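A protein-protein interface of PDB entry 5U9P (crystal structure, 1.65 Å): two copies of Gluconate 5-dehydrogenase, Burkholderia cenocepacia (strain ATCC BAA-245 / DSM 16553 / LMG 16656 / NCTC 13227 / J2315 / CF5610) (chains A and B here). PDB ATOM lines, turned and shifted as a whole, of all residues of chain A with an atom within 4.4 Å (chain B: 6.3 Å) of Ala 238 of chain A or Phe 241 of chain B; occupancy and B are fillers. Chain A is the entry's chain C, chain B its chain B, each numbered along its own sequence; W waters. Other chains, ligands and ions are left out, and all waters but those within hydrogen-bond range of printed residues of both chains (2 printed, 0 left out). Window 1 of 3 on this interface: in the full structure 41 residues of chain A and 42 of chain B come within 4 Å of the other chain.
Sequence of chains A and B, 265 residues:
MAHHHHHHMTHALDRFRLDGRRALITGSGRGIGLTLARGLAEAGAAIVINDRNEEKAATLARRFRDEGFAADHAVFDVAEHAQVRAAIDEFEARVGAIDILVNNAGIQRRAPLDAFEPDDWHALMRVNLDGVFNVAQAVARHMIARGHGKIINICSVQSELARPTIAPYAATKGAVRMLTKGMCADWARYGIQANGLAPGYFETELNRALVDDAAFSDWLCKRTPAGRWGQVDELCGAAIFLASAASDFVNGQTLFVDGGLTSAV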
ATOM      1  N   LEU A 197      26.928  -6.109  31.051  1.00  0.00           N
ATOM      2  CA  LEU A 197      25.965  -6.420  29.995  1.00  0.00           C
ATOM      3  C   LEU A 197      24.606  -6.103  30.608  1.00  0.00           C
ATOM      4  O   LEU A 197      24.188  -6.771  31.561  1.00  0.00           O
ATOM      5  CB  LEU A 197      26.095  -7.885  29.550  1.00  0.00           C
ATOM      6  CG  LEU A 197      25.370  -8.387  28.290  1.00  0.00           C
ATOM      7  CD1 LEU A 197      25.792  -9.839  28.006  1.00  0.00           C
ATOM      8  CD2 LEU A 197      23.867  -8.329  28.453  1.00  0.00           C
ATOM      9  N   LEU A 235      20.814 -12.098  23.940  1.00  0.00           N
ATOM     10  CA  LEU A 235      21.879 -11.674  24.835  1.00  0.00           C
ATOM     11  C   LEU A 235      23.179 -12.452  24.621  1.00  0.00           C
ATOM     12  O   LEU A 235      24.227 -12.023  25.109  1.00  0.00           O
ATOM     13  CB  LEU A 235      21.421 -11.848  26.298  1.00  0.00           C
ATOM     14  CG  LEU A 235      20.181 -11.025  26.683  1.00  0.00           C
ATOM     15  CD1 LEU A 235      19.536 -11.489  28.000  1.00  0.00           C
ATOM     16  CD2 LEU A 235      20.520  -9.512  26.768  1.00  0.00           C
ATOM     17  N   CYS A 236      23.143 -13.570  23.888  1.00  0.00           N
ATOM     18  CA  CYS A 236      24.336 -14.409  23.775  1.00  0.00           C
ATOM     19  C   CYS A 236      25.445 -13.713  23.002  1.00  0.00           C
ATOM     20  O   CYS A 236      26.628 -13.864  23.341  1.00  0.00           O
ATOM     21  CB  CYS A 236      24.001 -15.740  23.108  1.00  0.00           C
ATOM     22  SG  CYS A 236      22.926 -16.735  24.145  1.00  0.00           S
ATOM     23  N   GLY A 237      25.095 -12.975  21.953  1.00  0.00           N
ATOM     24  CA  GLY A 237      26.125 -12.333  21.150  1.00  0.00           C
ATOM     25  C   GLY A 237      26.968 -11.384  21.972  1.00  0.00           C
ATOM     26  O   GLY A 237      28.208 -11.416  21.916  1.00  0.00           O
ATOM     27  N   ALA A 238      26.304 -10.520  22.753  1.00  0.00           N
ATOM     28  CA  ALA A 238      27.033  -9.565  23.588  1.00  0.00           C
ATOM     29  C   ALA A 238      27.913 -10.277  24.602  1.00  0.00           C
ATOM     30  O   ALA A 238      29.034  -9.833  24.876  1.00  0.00           O
ATOM     31  CB  ALA A 238      26.060  -8.628  24.314  1.00  0.00           C
ATOM     32  N   ALA A 239      27.417 -11.376  25.177  1.00  0.00           N
ATOM     33  CA  ALA A 239      28.201 -12.122  26.163  1.00  0.00           C
ATOM     34  C   ALA A 239      29.424 -12.762  25.516  1.00  0.00           C
ATOM     35  O   ALA A 239      30.532 -12.689  26.065  1.00  0.00           O
ATOM     36  CB  ALA A 239      27.334 -13.192  26.838  1.00  0.00           C
ATOM     37  N   ILE A 240      29.250 -13.354  24.329  1.00  0.00           N
ATOM     38  CA  ILE A 240      30.379 -13.965  23.628  1.00  0.00           C
ATOM     39  C   ILE A 240      31.405 -12.899  23.260  1.00  0.00           C
ATOM     40  O   ILE A 240      32.610 -13.094  23.434  1.00  0.00           O
ATOM     41  CB  ILE A 240      29.893 -14.733  22.381  1.00  0.00           C
ATOM     42  CG1 ILE A 240      29.090 -15.982  22.795  1.00  0.00           C
ATOM     43  CG2 ILE A 240      31.079 -15.074  21.472  1.00  0.00           C
ATOM     44  CD1 ILE A 240      28.212 -16.528  21.634  1.00  0.00           C
ATOM     45  N   PHE A 241      30.937 -11.741  22.773  1.00  0.00           N
ATOM     46  CA  PHE A 241      31.845 -10.644  22.438  1.00  0.00           C
ATOM     47  C   PHE A 241      32.680 -10.212  23.648  1.00  0.00           C
ATOM     48  O   PHE A 241      33.915 -10.163  23.581  1.00  0.00           O
ATOM     49  CB  PHE A 241      31.030  -9.475  21.868  1.00  0.00           C
ATOM     50  CG  PHE A 241      31.841  -8.200  21.676  1.00  0.00           C
ATOM     51  CD1 PHE A 241      32.797  -8.110  20.674  1.00  0.00           C
ATOM     52  CD2 PHE A 241      31.683  -7.117  22.534  1.00  0.00           C
ATOM     53  CE1 PHE A 241      33.551  -6.965  20.509  1.00  0.00           C
ATOM     54  CE2 PHE A 241      32.445  -5.958  22.352  1.00  0.00           C
ATOM     55  CZ  PHE A 241      33.370  -5.886  21.333  1.00  0.00           C
ATOM     56  N   LEU A 242      32.020  -9.929  24.773  1.00  0.00           N
ATOM     57  CA  LEU A 242      32.724  -9.475  25.970  1.00  0.00           C
ATOM     58  C   LEU A 242      33.571 -10.568  26.613  1.00  0.00           C
ATOM     59  O   LEU A 242      34.470 -10.249  27.395  1.00  0.00           O
ATOM     60  CB  LEU A 242      31.718  -8.938  26.997  1.00  0.00           C
ATOM     61  CG  LEU A 242      30.953  -7.691  26.506  1.00  0.00           C
ATOM     62  CD1 LEU A 242      29.856  -7.380  27.522  1.00  0.00           C
ATOM     63  CD2 LEU A 242      31.895  -6.475  26.322  1.00  0.00           C
ATOM     64  N   LEU A 255      27.349  -2.471  28.218  1.00  0.00           N
ATOM     65  CA  LEU A 255      26.681  -2.553  26.920  1.00  0.00           C
ATOM     66  C   LEU A 255      25.212  -2.877  27.156  1.00  0.00           C
ATOM     67  O   LEU A 255      24.899  -3.911  27.745  1.00  0.00           O
ATOM     68  CB  LEU A 255      27.323  -3.640  26.058  1.00  0.00           C
ATOM     69  CG  LEU A 255      26.630  -3.942  24.723  1.00  0.00           C
ATOM     70  CD1 LEU A 255      26.599  -2.713  23.867  1.00  0.00           C
ATOM     71  CD2 LEU A 255      27.361  -5.070  24.029  1.00  0.00           C
ATOM     72  N   VAL A 257      21.573  -4.002  25.966  1.00  0.00           N
ATOM     73  CA  VAL A 257      20.957  -4.830  24.923  1.00  0.00           C
ATOM     74  C   VAL A 257      19.451  -4.760  25.154  1.00  0.00           C
ATOM     75  O   VAL A 257      18.871  -5.602  25.844  1.00  0.00           O
ATOM     76  CB  VAL A 257      21.466  -6.274  24.952  1.00  0.00           C
ATOM     77  CG1 VAL A 257      20.931  -7.060  23.730  1.00  0.00           C
ATOM     78  CG2 VAL A 257      23.000  -6.278  24.983  1.00  0.00           C
ATOM     79  N   PHE B  16      27.590 -14.326  14.168  1.00  0.00           N
ATOM     80  CA  PHE B  16      28.532 -13.239  13.897  1.00  0.00           C
ATOM     81  C   PHE B  16      28.923 -13.161  12.423  1.00  0.00           C
ATOM     82  O   PHE B  16      29.577 -12.195  12.023  1.00  0.00           O
ATOM     83  CB  PHE B  16      29.808 -13.404  14.742  1.00  0.00           C
ATOM     84  CG  PHE B  16      29.629 -13.115  16.209  1.00  0.00           C
ATOM     85  CD1 PHE B  16      30.003 -11.889  16.723  1.00  0.00           C
ATOM     86  CD2 PHE B  16      29.096 -14.065  17.079  1.00  0.00           C
ATOM     87  CE1 PHE B  16      29.858 -11.594  18.066  1.00  0.00           C
ATOM     88  CE2 PHE B  16      28.940 -13.770  18.427  1.00  0.00           C
ATOM     89  CZ  PHE B  16      29.323 -12.529  18.921  1.00  0.00           C
ATOM     90  N   LEU B  18      28.745 -12.559   8.412  1.00  0.00           N
ATOM     91  CA  LEU B  18      28.088 -11.522   7.618  1.00  0.00           C
ATOM     92  C   LEU B  18      27.798 -11.980   6.190  1.00  0.00           C
ATOM     93  O   LEU B  18      27.514 -11.146   5.321  1.00  0.00           O
ATOM     94  CB  LEU B  18      28.948 -10.249   7.602  1.00  0.00           C
ATOM     95  CG  LEU B  18      29.331  -9.642   8.962  1.00  0.00           C
ATOM     96  CD1 LEU B  18      30.216  -8.388   8.789  1.00  0.00           C
ATOM     97  CD2 LEU B  18      28.125  -9.305   9.828  1.00  0.00           C
ATOM     98  N   LYS B 150      21.803  -2.307   9.102  1.00  0.00           N
ATOM     99  CA  LYS B 150      22.706  -1.904  10.181  1.00  0.00           C
ATOM    100  C   LYS B 150      23.353  -0.582   9.816  1.00  0.00           C
ATOM    101  O   LYS B 150      23.870  -0.433   8.707  1.00  0.00           O
ATOM    102  CB  LYS B 150      23.818  -2.924  10.407  1.00  0.00           C
ATOM    103  CG  LYS B 150      23.343  -4.318  10.682  1.00  0.00           C
ATOM    104  CD  LYS B 150      22.726  -4.371  12.103  1.00  0.00           C
ATOM    105  CE  LYS B 150      22.710  -5.813  12.581  1.00  0.00           C
ATOM    106  NZ  LYS B 150      22.018  -5.990  13.916  1.00  0.00           N
ATOM    107  N   ILE B 152      26.364   1.876  11.523  1.00  0.00           N
ATOM    108  CA  ILE B 152      27.406   1.980  12.537  1.00  0.00           C
ATOM    109  C   ILE B 152      28.102   3.321  12.330  1.00  0.00           C
ATOM    110  O   ILE B 152      28.770   3.527  11.311  1.00  0.00           O
ATOM    111  CB  ILE B 152      28.408   0.820  12.437  1.00  0.00           C
ATOM    112  CG1 ILE B 152      27.709  -0.526  12.665  1.00  0.00           C
ATOM    113  CG2 ILE B 152      29.550   1.022  13.455  1.00  0.00           C
ATOM    114  CD1 ILE B 152      28.604  -1.735  12.286  1.00  0.00           C
ATOM    115  N   CYS B 236      38.012  -4.308  14.896  1.00  0.00           N
ATOM    116  CA  CYS B 236      37.275  -5.135  13.946  1.00  0.00           C
ATOM    117  C   CYS B 236      36.215  -5.975  14.640  1.00  0.00           C
ATOM    118  O   CYS B 236      35.101  -6.123  14.123  1.00  0.00           O
ATOM    119  CB  CYS B 236      38.239  -6.027  13.166  1.00  0.00           C
ATOM    120  SG  CYS B 236      39.202  -5.123  11.987  1.00  0.00           S
ATOM    121  N   GLY B 237      36.534  -6.530  15.812  1.00  0.00           N
ATOM    122  CA  GLY B 237      35.560  -7.372  16.491  1.00  0.00           C
ATOM    123  C   GLY B 237      34.270  -6.636  16.803  1.00  0.00           C
ATOM    124  O   GLY B 237      33.176  -7.157  16.590  1.00  0.00           O
ATOM    125  N   ALA B 238      34.385  -5.413  17.346  1.00  0.00           N
ATOM    126  CA  ALA B 238      33.207  -4.613  17.670  1.00  0.00           C
ATOM    127  C   ALA B 238      32.405  -4.273  16.414  1.00  0.00           C
ATOM    128  O   ALA B 238      31.166  -4.280  16.431  1.00  0.00           O
ATOM    129  CB  ALA B 238      33.635  -3.318  18.379  1.00  0.00           C
ATOM    130  N   ALA B 239      33.094  -3.937  15.321  1.00  0.00           N
ATOM    131  CA  ALA B 239      32.387  -3.588  14.088  1.00  0.00           C
ATOM    132  C   ALA B 239      31.615  -4.783  13.544  1.00  0.00           C
ATOM    133  O   ALA B 239      30.438  -4.669  13.169  1.00  0.00           O
ATOM    134  CB  ALA B 239      33.376  -3.064  13.033  1.00  0.00           C
ATOM    135  N   ILE B 240      32.260  -5.954  13.510  1.00  0.00           N
ATOM    136  CA  ILE B 240      31.587  -7.164  13.053  1.00  0.00           C
ATOM    137  C   ILE B 240      30.374  -7.462  13.932  1.00  0.00           C
ATOM    138  O   ILE B 240      29.285  -7.747  13.436  1.00  0.00           O
ATOM    139  CB  ILE B 240      32.582  -8.336  13.040  1.00  0.00           C
ATOM    140  CG1 ILE B 240      33.685  -8.094  11.996  1.00  0.00           C
ATOM    141  CG2 ILE B 240      31.845  -9.682  12.829  1.00  0.00           C
ATOM    142  CD1 ILE B 240      34.862  -9.069  12.132  1.00  0.00           C
ATOM    143  N   PHE B 241      30.551  -7.402  15.254  1.00  0.00           N
ATOM    144  CA  PHE B 241      29.439  -7.634  16.177  1.00  0.00           C
ATOM    145  C   PHE B 241      28.257  -6.713  15.879  1.00  0.00           C
ATOM    146  O   PHE B 241      27.113  -7.166  15.747  1.00  0.00           O
ATOM    147  CB  PHE B 241      29.936  -7.431  17.610  1.00  0.00           C
ATOM    148  CG  PHE B 241      28.841  -7.377  18.637  1.00  0.00           C
ATOM    149  CD1 PHE B 241      28.039  -8.486  18.855  1.00  0.00           C
ATOM    150  CD2 PHE B 241      28.630  -6.225  19.401  1.00  0.00           C
ATOM    151  CE1 PHE B 241      27.029  -8.450  19.815  1.00  0.00           C
ATOM    152  CE2 PHE B 241      27.613  -6.186  20.363  1.00  0.00           C
ATOM    153  CZ  PHE B 241      26.824  -7.301  20.561  1.00  0.00           C
ATOM    154  N   LEU B 242      28.522  -5.413  15.743  1.00  0.00           N
ATOM    155  CA  LEU B 242      27.443  -4.459  15.504  1.00  0.00           C
ATOM    156  C   LEU B 242      26.828  -4.604  14.119  1.00  0.00           C
ATOM    157  O   LEU B 242      25.687  -4.179  13.908  1.00  0.00           O
ATOM    158  CB  LEU B 242      27.969  -3.030  15.706  1.00  0.00           C
ATOM    159  CG  LEU B 242      28.297  -2.698  17.161  1.00  0.00           C
ATOM    160  CD1 LEU B 242      28.911  -1.283  17.209  1.00  0.00           C
ATOM    161  CD2 LEU B 242      27.047  -2.814  18.067  1.00  0.00           C
ATOM    162  N   ALA B 243      27.552  -5.199  13.174  1.00  0.00           N
ATOM    163  CA  ALA B 243      27.040  -5.398  11.834  1.00  0.00           C
ATOM    164  C   ALA B 243      26.261  -6.704  11.685  1.00  0.00           C
ATOM    165  O   ALA B 243      25.614  -6.903  10.653  1.00  0.00           O
ATOM    166  CB  ALA B 243      28.211  -5.373  10.837  1.00  0.00           C
ATOM    167  N   SER B 244      26.295  -7.581  12.690  1.00  0.00           N
ATOM    168  CA  SER B 244      25.831  -8.957  12.561  1.00  0.00           C
ATOM    169  C   SER B 244      24.484  -9.184  13.239  1.00  0.00           C
ATOM    170  O   SER B 244      24.004  -8.362  14.025  1.00  0.00           O
ATOM    171  CB  SER B 244      26.866  -9.918  13.152  1.00  0.00           C
ATOM    172  OG  SER B 244      26.862  -9.871  14.570  1.00  0.00           O
ATOM    173  N   ALA B 245      23.905 -10.364  12.961  1.00  0.00           N
ATOM    174  CA  ALA B 245      22.681 -10.771  13.653  1.00  0.00           C
ATOM    175  C   ALA B 245      22.895 -10.944  15.156  1.00  0.00           C
ATOM    176  O   ALA B 245      21.927 -10.909  15.932  1.00  0.00           O
ATOM    177  CB  ALA B 245      22.155 -12.077  13.040  1.00  0.00           C
ATOM    178  N   ALA B 246      24.141 -11.123  15.587  1.00  0.00           N
ATOM    179  CA  ALA B 246      24.438 -11.303  17.002  1.00  0.00           C
ATOM    180  C   ALA B 246      24.124 -10.064  17.841  1.00  0.00           C
ATOM    181  O   ALA B 246      24.125 -10.161  19.078  1.00  0.00           O
ATOM    182  CB  ALA B 246      25.918 -11.680  17.163  1.00  0.00           C
ATOM    183  N   SER B 247      23.850  -8.917  17.208  1.00  0.00           N
ATOM    184  CA  SER B 247      23.504  -7.677  17.900  1.00  0.00           C
ATOM    185  C   SER B 247      22.142  -7.129  17.473  1.00  0.00           C
ATOM    186  O   SER B 247      21.887  -5.928  17.628  1.00  0.00           O
ATOM    187  CB  SER B 247      24.576  -6.610  17.671  1.00  0.00           C
ATOM    188  OG  SER B 247      24.581  -6.237  16.292  1.00  0.00           O
ATOM    189  N   ASP B 248      21.226  -7.994  17.017  1.00  0.00           N
ATOM    190  CA  ASP B 248      19.946  -7.502  16.500  1.00  0.00           C
ATOM    191  C   ASP B 248      19.092  -6.773  17.545  1.00  0.00           C
ATOM    192  O   ASP B 248      18.246  -5.951  17.160  1.00  0.00           O
ATOM    193  CB  ASP B 248      19.133  -8.659  15.890  1.00  0.00           C
ATOM    194  CG  ASP B 248      19.539  -8.974  14.445  1.00  0.00           C
ATOM    195  OD1 ASP B 248      20.447  -8.324  13.892  1.00  0.00           O
ATOM    196  OD2 ASP B 248      18.923  -9.882  13.846  1.00  0.00           O
ATOM    197  N   VAL B 250      20.538  -4.856  19.956  1.00  0.00           N
ATOM    198  CA  VAL B 250      21.342  -3.697  20.352  1.00  0.00           C
ATOM    199  C   VAL B 250      20.961  -2.540  19.429  1.00  0.00           C
ATOM    200  O   VAL B 250      21.094  -2.660  18.207  1.00  0.00           O
ATOM    201  CB  VAL B 250      22.849  -3.994  20.239  1.00  0.00           C
ATOM    202  CG1 VAL B 250      23.672  -2.765  20.685  1.00  0.00           C
ATOM    203  CG2 VAL B 250      23.206  -5.220  21.050  1.00  0.00           C
ATOM    204  N   LEU B 255      29.180   2.034  21.737  1.00  0.00           N
ATOM    205  CA  LEU B 255      30.129   1.122  22.384  1.00  0.00           C
ATOM    206  C   LEU B 255      31.525   1.746  22.347  1.00  0.00           C
ATOM    207  O   LEU B 255      32.081   1.983  21.262  1.00  0.00           O
ATOM    208  CB  LEU B 255      30.124  -0.233  21.673  1.00  0.00           C
ATOM    209  CG  LEU B 255      31.201  -1.238  22.141  1.00  0.00           C
ATOM    210  CD1 LEU B 255      31.065  -1.580  23.645  1.00  0.00           C
ATOM    211  CD2 LEU B 255      31.175  -2.489  21.249  1.00  0.00           C
HETATM  212  O   HOH W   1      23.793  -9.662  21.786  1.00  0.00           O
HETATM  213  O   HOH W   2      22.720 -12.990  20.263  1.00  0.00           O
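OG of Ser 244 of chain B sits close to N of Ala 246 of chain B, 3.2 Å away.
OG of Ser 244 of chain B sits at hydrogen-bond distance from O of Phe 241 of chain B, 3.0 Å away.
The backbone carbonyl oxygen (O) of Phe 241 of chain B lies within hydrogen-bond range of the side-chain hydroxyl (OG) of Ser 247 of chain B (2.8 Å).
Phe 16 of chain B touches Gly 237 of chain A.
Gly 237 of chain A touches Phe 241 of chain B (C to CE1, 3.6 Å).
Ala 246 of chain B touches Gly 237 of chain A (O to CA, 3.6 Å).
Phe 241 of chain B touches Ala 238 of chain A (CE1 to N, 3.7 Å).
CG2 of Ile 240 of chain A touches CE2 of Phe 16 of chain B (3.9 Å).
Phe 241 of chain A touches Gly 237 of chain B.
Phe 241 of chain A touches Ala 238 of chain B.
Leu 255 of chain B touches Phe 241 of chain A.
CD2 of Leu 255 of chain A touches CE2 of Phe 241 of chain B, at 3.8 Å.
CG2 of Val 250 of chain B touches CG1 of Val 257 of chain A, at 3.97 Å.
Leu 197 of chain A touches none of the printed residues of chain B.
Ala 238 of chain A touches just one residue of chain B: Phe 241 (3.7 Å).
Of the printed residues of chain B, Phe 241 of chain A touches Gly 237 (3.8 Å), Ala 238 (3.6 Å) and Leu 255 (3.9 Å).
Printed residues of chain A within 4 Å of Gly 237 of chain B: Phe 241.
Of the printed residues of chain A, Ala 238 of chain B touches Phe 241.
Phe 241 of chain B touches just these residues of chain A: Gly 237, Ala 238 and Leu 255.
Leu 242 of chain B touches none of the printed residues of chain A.
Of the printed residues of chain A, Ala 246 of chain B touches Gly 237 (3.6 Å).
The nearest residue of chain B that does not touch Ala 238 of chain A is Ala 246 of chain B (4.3 Å).
The nearest residue of chain A that does not touch Phe 241 of chain B is Phe 241 of chain A (4.2 Å).
The nearest printed residue of chain A that does not touch Leu 255 of chain B is Leu 255 of chain A (4.6 Å).
Of the 19 printed residues of chain B, 7 touch a printed residue of chain A.
Hydrophobic or aromatic side chains of chain B within 4 Å of the printed part of chain A: Phe 16, Ala 238, Phe 241, Val 250 and Leu 255.
Printed residues of chain A that touch a printed residue of chain B: Gly 237, Ala 238, Ile 240, Phe 241, Leu 255 and Val 257.
Along chain A the printed residues that touch a printed residue of chain B span positions 237 to 257.
Among the printed residues, 10 pairs touch across the chains.
Among the printed residues, no Asp or Glu carboxylate lies within 4 Å of a Lys or Arg side-chain nitrogen of the other chain.
Gly 237 of chain A touches Phe 241 of chain B, and with the chains exchanged Phe 241 of chain A touches Gly 237 of chain B.
Ala 238 of chain A touches Phe 241 of chain B, and with the chains exchanged Phe 241 of chain A touches Ala 238 of chain B.
Phe 241 of chain A touches Leu 255 of chain B, and with the chains exchanged Leu 255 of chain A touches Phe 241 of chain B.
Of the 10 pairs that touch across the chains among the printed residues, 6 have their exchanged pair printed and touching as well.
Water W1 bridges O of Ala 246 of chain B and N of Ala 238 of chain A.
Water W2 bridges N of Gly 237 of chain A (2.9 Å) and O of Ala 246 of chain B (3.4 Å).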
